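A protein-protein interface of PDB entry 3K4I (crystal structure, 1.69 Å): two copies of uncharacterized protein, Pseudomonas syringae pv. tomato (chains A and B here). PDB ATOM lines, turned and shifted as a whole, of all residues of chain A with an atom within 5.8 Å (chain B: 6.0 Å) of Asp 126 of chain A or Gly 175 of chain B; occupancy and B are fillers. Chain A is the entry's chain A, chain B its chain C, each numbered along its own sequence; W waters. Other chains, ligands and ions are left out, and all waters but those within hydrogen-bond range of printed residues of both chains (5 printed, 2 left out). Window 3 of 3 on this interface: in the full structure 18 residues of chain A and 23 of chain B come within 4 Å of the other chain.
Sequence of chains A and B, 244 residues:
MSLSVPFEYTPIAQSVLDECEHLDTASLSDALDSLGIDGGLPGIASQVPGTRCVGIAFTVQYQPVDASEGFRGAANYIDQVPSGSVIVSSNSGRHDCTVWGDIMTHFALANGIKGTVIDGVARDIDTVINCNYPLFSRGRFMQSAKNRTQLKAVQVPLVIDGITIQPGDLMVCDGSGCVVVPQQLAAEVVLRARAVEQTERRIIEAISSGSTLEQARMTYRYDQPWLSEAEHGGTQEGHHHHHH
The backbone NH (N) of Asp 124 of chain A lies within hydrogen-bond range of the side-chain hydroxyl (OG) of Ser 176 of chain B (3.0 Å). The backbone NH (N) of Ile 125 of chain A sits at hydrogen-bond distance from the side-chain hydroxyl (OG) of Ser 176 of chain B (3.1 Å). The side-chain carboxylate of Asp 126 of chain A sits at hydrogen-bond distance from the backbone NH of Gly 175 of chain B (2.9 Å).
The side-chain carboxylate (OD1) of Asp 174 of chain B sits at hydrogen-bond distance from the side-chain hydroxyl (OG1) of Thr 25 of chain B, at 2.6 Å. OD1 of Asp 174 of chain B is in hydrogen-bond range of N of Ser 176 of chain B (3.0 Å).
Asp 126 of chain A touches Asp 174 of chain B (OD2 to CB, 3.6 Å). Gly 175 of chain B touches Arg 140 of chain A. C of Arg 140 of chain A touches O of Ser 176 of chain B, 3.8 Å away.
Asp 126 of chain A touches just these residues of chain B: Asp 174 (3.6 Å) and Gly 175 (2.9 Å). Of the printed residues of chain A, Gly 175 of chain B touches Asp 126 (2.9 Å) and Arg 140 (3.6 Å). Printed residues of chain A within 4 Å of Asp 174 of chain B: Asp 126. Printed residues of chain B within 4 Å of Arg 140 of chain A: Gly 175 (3.6 Å) and Ser 176 (3.8 Å). Of the printed residues of chain B, Asp 124 of chain A touches Ser 176 (3.0 Å). Of the printed residues of chain A, Ser 176 of chain B touches Asp 124 (3.0 Å), Ile 125 (3.1 Å) and Arg 140 (3.8 Å). Arg 52 of chain B touches none of the printed residues of chain A. The nearest printed residue of chain A that does not touch Gly 175 of chain B is Ile 125 of chain A (4.001 Å). The nearest printed residue of chain B that does not touch Asp 124 of chain A is Thr 25 of chain B (6.0 Å).
Hydrophobic or aromatic side chains of chain A that line the printed part of chain B: Ile 125. Among the printed residues, 6 pairs touch across the chains. Among the printed residues, no Asp or Glu carboxylate lies within 4 Å of a Lys or Arg side-chain nitrogen of the other chain.
No position is printed for both chains.
Water W2 lies within hydrogen-bond range of the side-chain hydroxyl of Ser 176 of chain B (2.6 Å), the side-chain carboxylate of Asp 126 of chain A (2.9 Å) and the backbone NH of Ile 125 of chain A (3.2 Å). Water W4 bridges O of Thr 51 of chain B and OD2 of Asp 126 of chain A. Water W1 bridges O of Ser 46 of chain B (2.7 Å) and NH1 of Arg 140 of chain A (2.9 Å). Water W3 lies within hydrogen-bond range of the side-chain carboxylate (OD1) of Asp 126 of chain A and the backbone NH (N) of Gly 50 of chain B. Water W5 bridges the backbone carbonyl oxygen (O) of Arg 140 of chain A (2.9 Å) and the backbone carbonyl oxygen (O) of Ser 176 of chain B (3.0 Å).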
ATOM      1  N   ASP A 124       9.197  14.450  18.931  1.00  0.00           N
ATOM      2  CA  ASP A 124       7.966  14.885  18.257  1.00  0.00           C
ATOM      3  C   ASP A 124       8.110  16.262  17.615  1.00  0.00           C
ATOM      4  O   ASP A 124       7.206  17.108  17.698  1.00  0.00           O
ATOM      5  CB  ASP A 124       6.787  14.854  19.231  1.00  0.00           C
ATOM      6  CG  ASP A 124       6.476  13.478  19.703  1.00  0.00           C
ATOM      7  OD1 ASP A 124       6.534  12.542  18.868  1.00  0.00           O
ATOM      8  OD2 ASP A 124       6.120  13.306  20.881  1.00  0.00           O
ATOM      9  N   ILE A 125       9.235  16.453  16.934  1.00  0.00           N
ATOM     10  CA  ILE A 125       9.593  17.722  16.338  1.00  0.00           C
ATOM     11  C   ILE A 125       8.591  18.130  15.262  1.00  0.00           C
ATOM     12  O   ILE A 125       8.295  19.311  15.105  1.00  0.00           O
ATOM     13  CB  ILE A 125      11.010  17.699  15.766  1.00  0.00           C
ATOM     14  CG1 ILE A 125      12.006  17.199  16.824  1.00  0.00           C
ATOM     15  CG2 ILE A 125      11.431  19.112  15.337  1.00  0.00           C
ATOM     16  CD1 ILE A 125      12.116  18.099  18.063  1.00  0.00           C
ATOM     17  N   ASP A 126       8.045  17.147  14.559  1.00  0.00           N
ATOM     18  CA  ASP A 126       7.066  17.441  13.521  1.00  0.00           C
ATOM     19  C   ASP A 126       5.782  18.038  14.123  1.00  0.00           C
ATOM     20  O   ASP A 126       5.247  18.994  13.589  1.00  0.00           O
ATOM     21  CB  ASP A 126       6.835  16.225  12.643  1.00  0.00           C
ATOM     22  CG  ASP A 126       8.059  15.916  11.763  1.00  0.00           C
ATOM     23  OD1 ASP A 126       8.530  16.808  11.033  1.00  0.00           O
ATOM     24  OD2 ASP A 126       8.526  14.776  11.797  1.00  0.00           O
ATOM     25  N   THR A 127       5.338  17.511  15.266  1.00  0.00           N
ATOM     26  CA  THR A 127       4.193  18.099  15.992  1.00  0.00           C
ATOM     27  C   THR A 127       4.544  19.482  16.518  1.00  0.00           C
ATOM     28  O   THR A 127       3.739  20.406  16.456  1.00  0.00           O
ATOM     29  CB  THR A 127       3.763  17.164  17.170  1.00  0.00           C
ATOM     30  OG1 THR A 127       3.405  15.901  16.628  1.00  0.00           O
ATOM     31  CG2 THR A 127       2.593  17.732  17.928  1.00  0.00           C
ATOM     32  N   VAL A 128       5.751  19.627  17.075  1.00  0.00           N
ATOM     33  CA  VAL A 128       6.119  20.893  17.616  1.00  0.00           C
ATOM     34  C   VAL A 128       6.149  21.965  16.521  1.00  0.00           C
ATOM     35  O   VAL A 128       5.633  23.072  16.719  1.00  0.00           O
ATOM     36  CB  VAL A 128       7.477  20.836  18.378  1.00  0.00           C
ATOM     37  CG1 VAL A 128       7.730  22.160  19.003  1.00  0.00           C
ATOM     38  CG2 VAL A 128       7.448  19.722  19.454  1.00  0.00           C
ATOM     39  N   ILE A 129       6.711  21.626  15.355  1.00  0.00           N
ATOM     40  CA  ILE A 129       6.707  22.535  14.218  1.00  0.00           C
ATOM     41  C   ILE A 129       5.279  22.859  13.782  1.00  0.00           C
ATOM     42  O   ILE A 129       4.963  24.027  13.521  1.00  0.00           O
ATOM     43  CB  ILE A 129       7.497  21.949  13.036  1.00  0.00           C
ATOM     44  CG1 ILE A 129       8.993  21.967  13.382  1.00  0.00           C
ATOM     45  CG2 ILE A 129       7.230  22.706  11.722  1.00  0.00           C
ATOM     46  CD1 ILE A 129       9.819  21.090  12.446  1.00  0.00           C
ATOM     47  N   ASN A 130       4.419  21.842  13.738  1.00  0.00           N
ATOM     48  CA  ASN A 130       3.035  22.042  13.250  1.00  0.00           C
ATOM     49  C   ASN A 130       2.223  22.927  14.195  1.00  0.00           C
ATOM     50  O   ASN A 130       1.357  23.690  13.747  1.00  0.00           O
ATOM     51  CB  ASN A 130       2.304  20.715  13.117  1.00  0.00           C
ATOM     52  CG  ASN A 130       0.900  20.887  12.616  1.00  0.00           C
ATOM     53  OD1 ASN A 130       0.691  21.137  11.434  1.00  0.00           O
ATOM     54  ND2 ASN A 130      -0.077  20.779  13.515  1.00  0.00           N
ATOM     55  N   CYS A 131       2.493  22.806  15.499  1.00  0.00           N
ATOM     56  CA  CYS A 131       1.865  23.645  16.540  1.00  0.00           C
ATOM     57  C   CYS A 131       2.512  25.029  16.662  1.00  0.00           C
ATOM     58  O   CYS A 131       2.031  25.867  17.437  1.00  0.00           O
ATOM     59  CB  CYS A 131       1.946  22.970  17.917  1.00  0.00           C
ATOM     60  SG  CYS A 131       0.979  21.445  18.104  1.00  0.00           S
ATOM     61  N   ARG A 140      17.410  17.124  18.472  1.00  0.00           N
ATOM     62  CA  ARG A 140      16.198  16.357  18.240  1.00  0.00           C
ATOM     63  C   ARG A 140      16.519  14.870  18.355  1.00  0.00           C
ATOM     64  O   ARG A 140      17.559  14.382  17.860  1.00  0.00           O
ATOM     65  CB  ARG A 140      15.733  16.643  16.818  1.00  0.00           C
ATOM     66  CG  ARG A 140      15.418  18.109  16.528  1.00  0.00           C
ATOM     67  CD  ARG A 140      15.475  18.384  15.016  1.00  0.00           C
ATOM     68  NE  ARG A 140      14.898  19.686  14.717  1.00  0.00           N
ATOM     69  CZ  ARG A 140      14.406  20.027  13.535  1.00  0.00           C
ATOM     70  NH1 ARG A 140      14.424  19.151  12.510  1.00  0.00           N
ATOM     71  NH2 ARG A 140      13.857  21.213  13.391  1.00  0.00           N
ATOM     72  N   THR B  25       8.321   8.187  14.904  1.00  0.00           N
ATOM     73  CA  THR B  25       9.485   7.547  15.537  1.00  0.00           C
ATOM     74  C   THR B  25       9.330   7.380  17.040  1.00  0.00           C
ATOM     75  O   THR B  25       9.814   6.383  17.593  1.00  0.00           O
ATOM     76  CB  THR B  25      10.786   8.291  15.210  1.00  0.00           C
ATOM     77  OG1 THR B  25      10.606   9.686  15.455  1.00  0.00           O
ATOM     78  CG2 THR B  25      11.158   8.065  13.721  1.00  0.00           C
ATOM     79  N   SER B  46      17.424  14.482  10.535  1.00  0.00           N
ATOM     80  CA  SER B  46      16.739  14.871   9.322  1.00  0.00           C
ATOM     81  C   SER B  46      17.394  16.122   8.687  1.00  0.00           C
ATOM     82  O   SER B  46      17.559  17.161   9.344  1.00  0.00           O
ATOM     83  CB  SER B  46      15.264  15.133   9.621  1.00  0.00           C
ATOM     84  OG  SER B  46      14.658  15.621   8.444  1.00  0.00           O
ATOM     85  N   GLY B  50      10.303  18.442   6.844  1.00  0.00           N
ATOM     86  CA  GLY B  50       9.003  17.891   6.445  1.00  0.00           C
ATOM     87  C   GLY B  50       8.999  16.526   5.784  1.00  0.00           C
ATOM     88  O   GLY B  50       7.951  16.077   5.263  1.00  0.00           O
ATOM     89  N   THR B  51      10.150  15.864   5.770  1.00  0.00           N
ATOM     90  CA  THR B  51      10.232  14.532   5.160  1.00  0.00           C
ATOM     91  C   THR B  51      10.196  13.405   6.198  1.00  0.00           C
ATOM     92  O   THR B  51      10.439  13.619   7.401  1.00  0.00           O
ATOM     93  CB  THR B  51      11.488  14.369   4.283  1.00  0.00           C
ATOM     94  OG1 THR B  51      12.676  14.649   5.063  1.00  0.00           O
ATOM     95  CG2 THR B  51      11.388  15.291   3.042  1.00  0.00           C
ATOM     96  N   ARG B  52       9.881  12.215   5.717  1.00  0.00           N
ATOM     97  CA  ARG B  52       9.900  11.001   6.527  1.00  0.00           C
ATOM     98  C   ARG B  52      10.016   9.812   5.591  1.00  0.00           C
ATOM     99  O   ARG B  52       9.781   9.935   4.399  1.00  0.00           O
ATOM    100  CB  ARG B  52       8.636  10.907   7.414  1.00  0.00           C
ATOM    101  CG  ARG B  52       7.324  10.797   6.635  1.00  0.00           C
ATOM    102  CD  ARG B  52       6.114  10.843   7.581  1.00  0.00           C
ATOM    103  NE  ARG B  52       6.108   9.794   8.605  1.00  0.00           N
ATOM    104  CZ  ARG B  52       5.826   8.512   8.382  1.00  0.00           C
ATOM    105  NH1 ARG B  52       5.518   8.092   7.164  1.00  0.00           N
ATOM    106  NH2 ARG B  52       5.852   7.637   9.382  1.00  0.00           N
ATOM    107  N   PHE B 136      18.787  11.539   5.953  1.00  0.00           N
ATOM    108  CA  PHE B 136      19.141  11.685   7.345  1.00  0.00           C
ATOM    109  C   PHE B 136      20.627  11.446   7.471  1.00  0.00           C
ATOM    110  O   PHE B 136      21.139  10.460   6.927  1.00  0.00           O
ATOM    111  CB  PHE B 136      18.322  10.667   8.124  1.00  0.00           C
ATOM    112  CG  PHE B 136      16.861  10.832   7.913  1.00  0.00           C
ATOM    113  CD1 PHE B 136      16.097  11.591   8.801  1.00  0.00           C
ATOM    114  CD2 PHE B 136      16.246  10.288   6.789  1.00  0.00           C
ATOM    115  CE1 PHE B 136      14.732  11.769   8.591  1.00  0.00           C
ATOM    116  CE2 PHE B 136      14.864  10.499   6.548  1.00  0.00           C
ATOM    117  CZ  PHE B 136      14.117  11.243   7.456  1.00  0.00           C
ATOM    118  N   CYS B 173      11.953   6.919   9.835  1.00  0.00           N
ATOM    119  CA  CYS B 173      12.677   8.160  10.069  1.00  0.00           C
ATOM    120  C   CYS B 173      11.759   9.334   9.849  1.00  0.00           C
ATOM    121  O   CYS B 173      10.970   9.315   8.907  1.00  0.00           O
ATOM    122  CB  CYS B 173      13.843   8.286   9.078  1.00  0.00           C
ATOM    123  SG  CYS B 173      14.910   6.844   9.015  1.00  0.00           S
ATOM    124  N   ASP B 174      11.895  10.353  10.701  1.00  0.00           N
ATOM    125  CA  ASP B 174      11.158  11.609  10.557  1.00  0.00           C
ATOM    126  C   ASP B 174      11.942  12.775  11.152  1.00  0.00           C
ATOM    127  O   ASP B 174      13.174  12.678  11.335  1.00  0.00           O
ATOM    128  CB  ASP B 174       9.730  11.485  11.154  1.00  0.00           C
ATOM    129  CG  ASP B 174       9.713  11.140  12.655  1.00  0.00           C
ATOM    130  OD1 ASP B 174      10.714  11.339  13.390  1.00  0.00           O
ATOM    131  OD2 ASP B 174       8.658  10.668  13.122  1.00  0.00           O
ATOM    132  N   GLY B 175      11.260  13.879  11.441  1.00  0.00           N
ATOM    133  CA  GLY B 175      11.949  15.064  11.997  1.00  0.00           C
ATOM    134  C   GLY B 175      12.707  14.822  13.295  1.00  0.00           C
ATOM    135  O   GLY B 175      13.692  15.537  13.598  1.00  0.00           O
ATOM    136  N   SER B 176      12.284  13.810  14.055  1.00  0.00           N
ATOM    137  CA  SER B 176      12.942  13.495  15.322  1.00  0.00           C
ATOM    138  C   SER B 176      14.164  12.565  15.176  1.00  0.00           C
ATOM    139  O   SER B 176      14.872  12.313  16.155  1.00  0.00           O
ATOM    140  CB  SER B 176      11.910  12.917  16.304  1.00  0.00           C
ATOM    141  OG  SER B 176      10.850  13.851  16.502  1.00  0.00           O
ATOM    142  N   GLY B 177      14.420  12.088  13.958  1.00  0.00           N
ATOM    143  CA  GLY B 177      15.534  11.184  13.692  1.00  0.00           C
ATOM    144  C   GLY B 177      15.133   9.822  13.156  1.00  0.00           C
ATOM    145  O   GLY B 177      14.015   9.649  12.588  1.00  0.00           O
HETATM  146  O   HOH W   1      16.774  17.577  11.922  1.00  0.00           O
HETATM  147  O   HOH W   2       9.136  14.236  14.576  1.00  0.00           O
HETATM  148  O   HOH W   3      10.787  17.759   9.758  1.00  0.00           O
HETATM  149  O   HOH W   4       8.379  14.626   8.853  1.00  0.00           O
HETATM  150  O   HOH W   5      17.837  12.007  16.210  1.00  0.00           O
